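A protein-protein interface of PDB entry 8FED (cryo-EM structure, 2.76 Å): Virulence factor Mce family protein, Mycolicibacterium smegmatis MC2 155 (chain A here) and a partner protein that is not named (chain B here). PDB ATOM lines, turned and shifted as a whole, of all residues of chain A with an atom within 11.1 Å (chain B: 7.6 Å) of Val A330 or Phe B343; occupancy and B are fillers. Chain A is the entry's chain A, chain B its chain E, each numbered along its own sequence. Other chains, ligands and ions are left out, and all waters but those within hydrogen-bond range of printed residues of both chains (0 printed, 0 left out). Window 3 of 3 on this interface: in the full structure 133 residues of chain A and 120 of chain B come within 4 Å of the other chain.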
ATOM      1  N   THR A 326     -29.286 -16.084  16.755  1.00  0.00           N
ATOM      2  CA  THR A 326     -29.157 -17.205  15.837  1.00  0.00           C
ATOM      3  C   THR A 326     -27.722 -17.294  15.337  1.00  0.00           C
ATOM      4  O   THR A 326     -27.004 -16.293  15.280  1.00  0.00           O
ATOM      5  CB  THR A 326     -30.107 -17.078  14.638  1.00  0.00           C
ATOM      6  OG1 THR A 326     -30.040 -15.748  14.111  1.00  0.00           O
ATOM      7  CG2 THR A 326     -31.541 -17.394  15.040  1.00  0.00           C
ATOM      8  N   ASN A 327     -27.314 -18.509  14.976  1.00  0.00           N
ATOM      9  CA  ASN A 327     -25.991 -18.779  14.422  1.00  0.00           C
ATOM     10  C   ASN A 327     -26.176 -19.114  12.947  1.00  0.00           C
ATOM     11  O   ASN A 327     -26.753 -20.153  12.611  1.00  0.00           O
ATOM     12  CB  ASN A 327     -25.309 -19.920  15.173  1.00  0.00           C
ATOM     13  CG  ASN A 327     -23.849 -19.641  15.449  1.00  0.00           C
ATOM     14  OD1 ASN A 327     -23.402 -18.497  15.386  1.00  0.00           O
ATOM     15  ND2 ASN A 327     -23.095 -20.689  15.762  1.00  0.00           N
ATOM     16  N   SER A 328     -25.677 -18.248  12.069  1.00  0.00           N
ATOM     17  CA  SER A 328     -25.994 -18.302  10.644  1.00  0.00           C
ATOM     18  C   SER A 328     -24.788 -18.808   9.861  1.00  0.00           C
ATOM     19  O   SER A 328     -23.802 -18.084   9.695  1.00  0.00           O
ATOM     20  CB  SER A 328     -26.431 -16.928  10.144  1.00  0.00           C
ATOM     21  OG  SER A 328     -27.536 -16.446  10.887  1.00  0.00           O
ATOM     22  N   LEU A 329     -24.881 -20.037   9.358  1.00  0.00           N
ATOM     23  CA  LEU A 329     -23.868 -20.610   8.484  1.00  0.00           C
ATOM     24  C   LEU A 329     -24.527 -21.098   7.203  1.00  0.00           C
ATOM     25  O   LEU A 329     -25.605 -21.696   7.239  1.00  0.00           O
ATOM     26  CB  LEU A 329     -23.119 -21.759   9.179  1.00  0.00           C
ATOM     27  CG  LEU A 329     -23.925 -22.926   9.759  1.00  0.00           C
ATOM     28  CD1 LEU A 329     -24.018 -24.088   8.781  1.00  0.00           C
ATOM     29  CD2 LEU A 329     -23.336 -23.384  11.084  1.00  0.00           C
ATOM     30  N   VAL A 330     -23.879 -20.833   6.070  1.00  0.00           N
ATOM     31  CA  VAL A 330     -24.446 -21.183   4.774  1.00  0.00           C
ATOM     32  C   VAL A 330     -24.247 -22.670   4.512  1.00  0.00           C
ATOM     33  O   VAL A 330     -23.246 -23.272   4.918  1.00  0.00           O
ATOM     34  CB  VAL A 330     -23.832 -20.315   3.657  1.00  0.00           C
ATOM     35  CG1 VAL A 330     -24.149 -18.848   3.898  1.00  0.00           C
ATOM     36  CG2 VAL A 330     -22.330 -20.523   3.576  1.00  0.00           C
ATOM     37  N   VAL A 331     -25.225 -23.281   3.845  1.00  0.00           N
ATOM     38  CA  VAL A 331     -25.231 -24.712   3.571  1.00  0.00           C
ATOM     39  C   VAL A 331     -26.005 -24.944   2.276  1.00  0.00           C
ATOM     40  O   VAL A 331     -26.634 -24.034   1.734  1.00  0.00           O
ATOM     41  CB  VAL A 331     -25.849 -25.510   4.745  1.00  0.00           C
ATOM     42  CG1 VAL A 331     -27.367 -25.468   4.689  1.00  0.00           C
ATOM     43  CG2 VAL A 331     -25.323 -26.941   4.790  1.00  0.00           C
ATOM     44  N   GLY A 332     -25.944 -26.172   1.765  1.00  0.00           N
ATOM     45  CA  GLY A 332     -26.710 -26.546   0.592  1.00  0.00           C
ATOM     46  C   GLY A 332     -28.035 -27.192   0.960  1.00  0.00           C
ATOM     47  O   GLY A 332     -28.189 -27.771   2.031  1.00  0.00           O
ATOM     48  N   VAL A 333     -28.999 -27.089   0.046  1.00  0.00           N
ATOM     49  CA  VAL A 333     -30.350 -27.574   0.288  1.00  0.00           C
ATOM     50  C   VAL A 333     -30.680 -28.672  -0.713  1.00  0.00           C
ATOM     51  O   VAL A 333     -30.112 -28.748  -1.804  1.00  0.00           O
ATOM     52  CB  VAL A 333     -31.393 -26.445   0.208  1.00  0.00           C
ATOM     53  CG1 VAL A 333     -31.315 -25.580   1.442  1.00  0.00           C
ATOM     54  CG2 VAL A 333     -31.171 -25.613  -1.042  1.00  0.00           C
ATOM     55  N   TYR A 383     -29.781 -38.428   1.822  1.00  0.00           N
ATOM     56  CA  TYR A 383     -28.838 -37.317   1.696  1.00  0.00           C
ATOM     57  C   TYR A 383     -27.547 -37.632   2.457  1.00  0.00           C
ATOM     58  O   TYR A 383     -27.178 -36.973   3.427  1.00  0.00           O
ATOM     59  CB  TYR A 383     -29.471 -36.025   2.191  1.00  0.00           C
ATOM     60  CG  TYR A 383     -30.511 -35.450   1.261  1.00  0.00           C
ATOM     61  CD1 TYR A 383     -30.153 -34.569   0.252  1.00  0.00           C
ATOM     62  CD2 TYR A 383     -31.853 -35.779   1.397  1.00  0.00           C
ATOM     63  CE1 TYR A 383     -31.097 -34.036  -0.598  1.00  0.00           C
ATOM     64  CE2 TYR A 383     -32.807 -35.249   0.550  1.00  0.00           C
ATOM     65  CZ  TYR A 383     -32.423 -34.378  -0.444  1.00  0.00           C
ATOM     66  OH  TYR A 383     -33.367 -33.848  -1.291  1.00  0.00           O
ATOM     67  N   ASN A 384     -26.861 -38.673   1.992  1.00  0.00           N
ATOM     68  CA  ASN A 384     -25.635 -39.151   2.612  1.00  0.00           C
ATOM     69  C   ASN A 384     -24.385 -38.728   1.854  1.00  0.00           C
ATOM     70  O   ASN A 384     -23.300 -39.243   2.136  1.00  0.00           O
ATOM     71  CB  ASN A 384     -25.667 -40.674   2.727  1.00  0.00           C
ATOM     72  CG  ASN A 384     -26.982 -41.184   3.261  1.00  0.00           C
ATOM     73  OD1 ASN A 384     -27.684 -40.479   3.982  1.00  0.00           O
ATOM     74  ND2 ASN A 384     -27.325 -42.419   2.912  1.00  0.00           N
ATOM     75  N   HIS A 385     -24.510 -37.809   0.900  1.00  0.00           N
ATOM     76  CA  HIS A 385     -23.391 -37.463   0.037  1.00  0.00           C
ATOM     77  C   HIS A 385     -23.606 -36.071  -0.532  1.00  0.00           C
ATOM     78  O   HIS A 385     -24.711 -35.523  -0.487  1.00  0.00           O
ATOM     79  CB  HIS A 385     -23.226 -38.486  -1.088  1.00  0.00           C
ATOM     80  CG  HIS A 385     -24.523 -38.922  -1.692  1.00  0.00           C
ATOM     81  ND1 HIS A 385     -25.398 -38.043  -2.290  1.00  0.00           N
ATOM     82  CD2 HIS A 385     -25.102 -40.144  -1.775  1.00  0.00           C
ATOM     83  CE1 HIS A 385     -26.457 -38.703  -2.723  1.00  0.00           C
ATOM     84  NE2 HIS A 385     -26.302 -39.980  -2.421  1.00  0.00           N
ATOM     85  N   PHE A 386     -22.529 -35.505  -1.068  1.00  0.00           N
ATOM     86  CA  PHE A 386     -22.574 -34.210  -1.738  1.00  0.00           C
ATOM     87  C   PHE A 386     -22.824 -34.448  -3.222  1.00  0.00           C
ATOM     88  O   PHE A 386     -21.968 -34.997  -3.923  1.00  0.00           O
ATOM     89  CB  PHE A 386     -21.273 -33.444  -1.508  1.00  0.00           C
ATOM     90  CG  PHE A 386     -21.142 -32.188  -2.329  1.00  0.00           C
ATOM     91  CD1 PHE A 386     -21.621 -30.983  -1.848  1.00  0.00           C
ATOM     92  CD2 PHE A 386     -20.511 -32.207  -3.563  1.00  0.00           C
ATOM     93  CE1 PHE A 386     -21.495 -29.827  -2.593  1.00  0.00           C
ATOM     94  CE2 PHE A 386     -20.385 -31.054  -4.312  1.00  0.00           C
ATOM     95  CZ  PHE A 386     -20.876 -29.863  -3.826  1.00  0.00           C
ATOM     96  N   GLU A 387     -23.996 -34.038  -3.700  1.00  0.00           N
ATOM     97  CA  GLU A 387     -24.346 -34.153  -5.106  1.00  0.00           C
ATOM     98  C   GLU A 387     -24.938 -32.843  -5.597  1.00  0.00           C
ATOM     99  O   GLU A 387     -25.560 -32.099  -4.835  1.00  0.00           O
ATOM    100  CB  GLU A 387     -25.336 -35.291  -5.358  1.00  0.00           C
ATOM    101  CG  GLU A 387     -24.717 -36.667  -5.263  1.00  0.00           C
ATOM    102  CD  GLU A 387     -25.564 -37.732  -5.919  1.00  0.00           C
ATOM    103  OE1 GLU A 387     -26.472 -37.376  -6.699  1.00  0.00           O
ATOM    104  OE2 GLU A 387     -25.321 -38.925  -5.653  1.00  0.00           O
ATOM    105  N   LEU A 388     -24.725 -32.568  -6.880  1.00  0.00           N
ATOM    106  CA  LEU A 388     -25.311 -31.390  -7.498  1.00  0.00           C
ATOM    107  C   LEU A 388     -26.827 -31.526  -7.573  1.00  0.00           C
ATOM    108  O   LEU A 388     -27.360 -32.619  -7.780  1.00  0.00           O
ATOM    109  CB  LEU A 388     -24.713 -31.176  -8.889  1.00  0.00           C
ATOM    110  CG  LEU A 388     -24.231 -32.419  -9.643  1.00  0.00           C
ATOM    111  CD1 LEU A 388     -25.380 -33.166 -10.306  1.00  0.00           C
ATOM    112  CD2 LEU A 388     -23.167 -32.047 -10.666  1.00  0.00           C
ATOM    113  N   LEU B 332     -23.094 -14.453  11.201  1.00  0.00           N
ATOM    114  CA  LEU B 332     -22.568 -15.147  10.027  1.00  0.00           C
ATOM    115  C   LEU B 332     -21.196 -15.707  10.374  1.00  0.00           C
ATOM    116  O   LEU B 332     -20.187 -15.003  10.292  1.00  0.00           O
ATOM    117  CB  LEU B 332     -22.495 -14.211   8.825  1.00  0.00           C
ATOM    118  CG  LEU B 332     -23.779 -13.589   8.263  1.00  0.00           C
ATOM    119  CD1 LEU B 332     -24.172 -12.313   9.001  1.00  0.00           C
ATOM    120  CD2 LEU B 332     -23.627 -13.318   6.776  1.00  0.00           C
ATOM    121  N   ASP B 333     -21.148 -16.978  10.765  1.00  0.00           N
ATOM    122  CA  ASP B 333     -19.900 -17.613  11.165  1.00  0.00           C
ATOM    123  C   ASP B 333     -19.296 -18.348   9.976  1.00  0.00           C
ATOM    124  O   ASP B 333     -19.979 -19.132   9.309  1.00  0.00           O
ATOM    125  CB  ASP B 333     -20.105 -18.568  12.343  1.00  0.00           C
ATOM    126  CG  ASP B 333     -21.037 -19.711  12.018  1.00  0.00           C
ATOM    127  OD1 ASP B 333     -22.040 -19.479  11.317  1.00  0.00           O
ATOM    128  OD2 ASP B 333     -20.760 -20.846  12.458  1.00  0.00           O
ATOM    129  N   LEU B 334     -18.022 -18.071   9.704  1.00  0.00           N
ATOM    130  CA  LEU B 334     -17.286 -18.696   8.612  1.00  0.00           C
ATOM    131  C   LEU B 334     -16.079 -19.468   9.133  1.00  0.00           C
ATOM    132  O   LEU B 334     -15.089 -19.643   8.420  1.00  0.00           O
ATOM    133  CB  LEU B 334     -16.858 -17.647   7.588  1.00  0.00           C
ATOM    134  CG  LEU B 334     -17.976 -16.744   7.064  1.00  0.00           C
ATOM    135  CD1 LEU B 334     -17.442 -15.765   6.032  1.00  0.00           C
ATOM    136  CD2 LEU B 334     -19.107 -17.573   6.482  1.00  0.00           C
ATOM    137  N   SER B 337     -14.768 -24.954  11.335  1.00  0.00           N
ATOM    138  CA  SER B 337     -15.670 -25.971  11.865  1.00  0.00           C
ATOM    139  C   SER B 337     -17.026 -25.911  11.172  1.00  0.00           C
ATOM    140  O   SER B 337     -17.574 -26.943  10.762  1.00  0.00           O
ATOM    141  CB  SER B 337     -15.828 -25.793  13.374  1.00  0.00           C
ATOM    142  OG  SER B 337     -16.337 -24.507  13.682  1.00  0.00           O
ATOM    143  N   SER B 338     -17.578 -24.703  11.029  1.00  0.00           N
ATOM    144  CA  SER B 338     -18.856 -24.543  10.346  1.00  0.00           C
ATOM    145  C   SER B 338     -18.751 -24.945   8.882  1.00  0.00           C
ATOM    146  O   SER B 338     -19.668 -25.568   8.335  1.00  0.00           O
ATOM    147  CB  SER B 338     -19.343 -23.101  10.475  1.00  0.00           C
ATOM    148  OG  SER B 338     -18.437 -22.202   9.859  1.00  0.00           O
ATOM    149  N   VAL B 339     -17.643 -24.588   8.229  1.00  0.00           N
ATOM    150  CA  VAL B 339     -17.444 -24.962   6.831  1.00  0.00           C
ATOM    151  C   VAL B 339     -17.342 -26.475   6.690  1.00  0.00           C
ATOM    152  O   VAL B 339     -17.922 -27.067   5.773  1.00  0.00           O
ATOM    153  CB  VAL B 339     -16.201 -24.252   6.265  1.00  0.00           C
ATOM    154  CG1 VAL B 339     -15.890 -24.749   4.865  1.00  0.00           C
ATOM    155  CG2 VAL B 339     -16.413 -22.750   6.262  1.00  0.00           C
ATOM    156  N   ASP B 340     -16.603 -27.124   7.593  1.00  0.00           N
ATOM    157  CA  ASP B 340     -16.444 -28.572   7.515  1.00  0.00           C
ATOM    158  C   ASP B 340     -17.764 -29.290   7.753  1.00  0.00           C
ATOM    159  O   ASP B 340     -18.064 -30.284   7.081  1.00  0.00           O
ATOM    160  CB  ASP B 340     -15.401 -29.051   8.519  1.00  0.00           C
ATOM    161  CG  ASP B 340     -15.158 -30.541   8.425  1.00  0.00           C
ATOM    162  OD1 ASP B 340     -14.603 -30.984   7.399  1.00  0.00           O
ATOM    163  OD2 ASP B 340     -15.525 -31.272   9.368  1.00  0.00           O
ATOM    164  N   ASN B 341     -18.555 -28.820   8.717  1.00  0.00           N
ATOM    165  CA  ASN B 341     -19.823 -29.485   8.996  1.00  0.00           C
ATOM    166  C   ASN B 341     -20.842 -29.223   7.894  1.00  0.00           C
ATOM    167  O   ASN B 341     -21.609 -30.119   7.525  1.00  0.00           O
ATOM    168  CB  ASN B 341     -20.367 -29.043  10.353  1.00  0.00           C
ATOM    169  CG  ASN B 341     -20.692 -30.216  11.255  1.00  0.00           C
ATOM    170  OD1 ASN B 341     -20.849 -31.346  10.791  1.00  0.00           O
ATOM    171  ND2 ASN B 341     -20.793 -29.956  12.552  1.00  0.00           N
ATOM    172  N   ALA B 342     -20.864 -28.001   7.356  1.00  0.00           N
ATOM    173  CA  ALA B 342     -21.892 -27.628   6.390  1.00  0.00           C
ATOM    174  C   ALA B 342     -21.665 -28.293   5.038  1.00  0.00           C
ATOM    175  O   ALA B 342     -22.596 -28.854   4.449  1.00  0.00           O
ATOM    176  CB  ALA B 342     -21.937 -26.109   6.241  1.00  0.00           C
ATOM    177  N   PHE B 343     -20.433 -28.254   4.529  1.00  0.00           N
ATOM    178  CA  PHE B 343     -20.163 -28.655   3.151  1.00  0.00           C
ATOM    179  C   PHE B 343     -19.528 -30.037   3.046  1.00  0.00           C
ATOM    180  O   PHE B 343     -20.057 -30.913   2.358  1.00  0.00           O
ATOM    181  CB  PHE B 343     -19.264 -27.617   2.468  1.00  0.00           C
ATOM    182  CG  PHE B 343     -19.913 -26.278   2.278  1.00  0.00           C
ATOM    183  CD1 PHE B 343     -21.029 -26.146   1.471  1.00  0.00           C
ATOM    184  CD2 PHE B 343     -19.400 -25.150   2.892  1.00  0.00           C
ATOM    185  CE1 PHE B 343     -21.626 -24.915   1.291  1.00  0.00           C
ATOM    186  CE2 PHE B 343     -19.994 -23.915   2.714  1.00  0.00           C
ATOM    187  CZ  PHE B 343     -21.106 -23.799   1.913  1.00  0.00           C
ATOM    188  N   LEU B 344     -18.403 -30.253   3.722  1.00  0.00           N
ATOM    189  CA  LEU B 344     -17.575 -31.427   3.484  1.00  0.00           C
ATOM    190  C   LEU B 344     -18.020 -32.655   4.271  1.00  0.00           C
ATOM    191  O   LEU B 344     -17.284 -33.645   4.311  1.00  0.00           O
ATOM    192  CB  LEU B 344     -16.112 -31.108   3.801  1.00  0.00           C
ATOM    193  CG  LEU B 344     -15.502 -29.923   3.050  1.00  0.00           C
ATOM    194  CD1 LEU B 344     -13.997 -29.918   3.210  1.00  0.00           C
ATOM    195  CD2 LEU B 344     -15.878 -29.949   1.577  1.00  0.00           C
ATOM    196  N   SER B 345     -19.194 -32.615   4.891  1.00  0.00           N
ATOM    197  CA  SER B 345     -19.672 -33.761   5.653  1.00  0.00           C
ATOM    198  C   SER B 345     -20.127 -34.877   4.721  1.00  0.00           C
ATOM    199  O   SER B 345     -20.677 -34.628   3.646  1.00  0.00           O
ATOM    200  CB  SER B 345     -20.819 -33.346   6.572  1.00  0.00           C
ATOM    201  OG  SER B 345     -20.418 -32.319   7.460  1.00  0.00           O
ATOM    202  N   GLY B 346     -19.887 -36.119   5.140  1.00  0.00           N
ATOM    203  CA  GLY B 346     -20.359 -37.278   4.414  1.00  0.00           C
ATOM    204  C   GLY B 346     -19.492 -37.730   3.261  1.00  0.00           C
ATOM    205  O   GLY B 346     -19.850 -38.704   2.586  1.00  0.00           O
ATOM    206  N   THR B 347     -18.368 -37.069   3.011  1.00  0.00           N
ATOM    207  CA  THR B 347     -17.476 -37.409   1.910  1.00  0.00           C
ATOM    208  C   THR B 347     -16.134 -37.886   2.466  1.00  0.00           C
ATOM    209  O   THR B 347     -15.956 -38.043   3.677  1.00  0.00           O
ATOM    210  CB  THR B 347     -17.304 -36.215   0.968  1.00  0.00           C
ATOM    211  OG1 THR B 347     -16.831 -35.082   1.707  1.00  0.00           O
ATOM    212  CG2 THR B 347     -18.626 -35.866   0.305  1.00  0.00           C
ATOM    213  N   VAL B 349     -13.333 -36.246   2.407  1.00  0.00           N
ATOM    214  CA  VAL B 349     -12.499 -35.151   2.890  1.00  0.00           C
ATOM    215  C   VAL B 349     -13.134 -34.550   4.135  1.00  0.00           C
ATOM    216  O   VAL B 349     -12.994 -33.351   4.400  1.00  0.00           O
ATOM    217  CB  VAL B 349     -12.294 -34.084   1.801  1.00  0.00           C
ATOM    218  CG1 VAL B 349     -11.422 -34.631   0.688  1.00  0.00           C
ATOM    219  CG2 VAL B 349     -13.634 -33.628   1.250  1.00  0.00           C
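The backbone carbonyl oxygen of Asp B333 lies within hydrogen-bond range of the side-chain hydroxyl of Ser B338, 3.5 Å away.
Of the 14 printed residues of chain A, 5 touch a printed residue of chain B. Hydrophobic or aromatic side chains of chain A that line the printed part of chain B: Leu A329, Val A330 and Val A331. Along chain A the printed residues that touch a printed residue of chain B span positions 328 to 384. Hydrophobic or aromatic side chains of chain B within 4 Å of the printed part of chain A: Ala B342 and Phe B343. Along chain B the printed residues that touch a printed residue of chain A span positions 332 to 346.
Of the printed residues of chain B, Ser A328 touches Leu B332 and Asp B333. Val A330 touches just these residues of chain B: Ala B342 and Phe B343. Of the printed residues of chain B, Val A331 touches Ala B342. Gly A332 touches none of the printed residues of chain B. Tyr A383 touches none of the printed residues of chain B. Of the printed residues of chain A, Leu B332 touches Ser A328 (3.2 Å). Of the printed residues of chain A, Asp B333 touches Ser A328 and Leu A329. No residue of chain A comes within 4 Å of Val B339. Ala B342 touches just these residues of chain A: Leu A329 (3.9 Å), Val A330 (3.4 Å) and Val A331 (3.3 Å). Phe B343 touches just one residue of chain A: Val A330. No residue of chain A comes within 4 Å of Leu B344. Of the printed residues of chain A, Gly B346 touches Asn A384. The nearest residue of chain A that does not touch Phe B343 is Val A331 (4.3 Å). The nearest printed residue of chain B that does not touch Leu A329 is Ser B338 (4.05 Å).
The backbone carbonyl oxygen (O) of Ser A328 lies within hydrogen-bond range of the backbone NH (N) of Asp B333. OD1 of Asp B333 lies close to N of Leu A329 (3.5 Å).
Among the printed residues, merely in contact across the chains: Ser A328 with Leu B332 (3.2 Å), Leu A329 with Ala B342 (3.9 Å), Val A330 with Ala B342 (3.4 Å), Val A330 with Phe B343 (3.7 Å), Val A331 with Ala B342 (3.3 Å) and Asn A384 with Gly B346 (3.5 Å).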
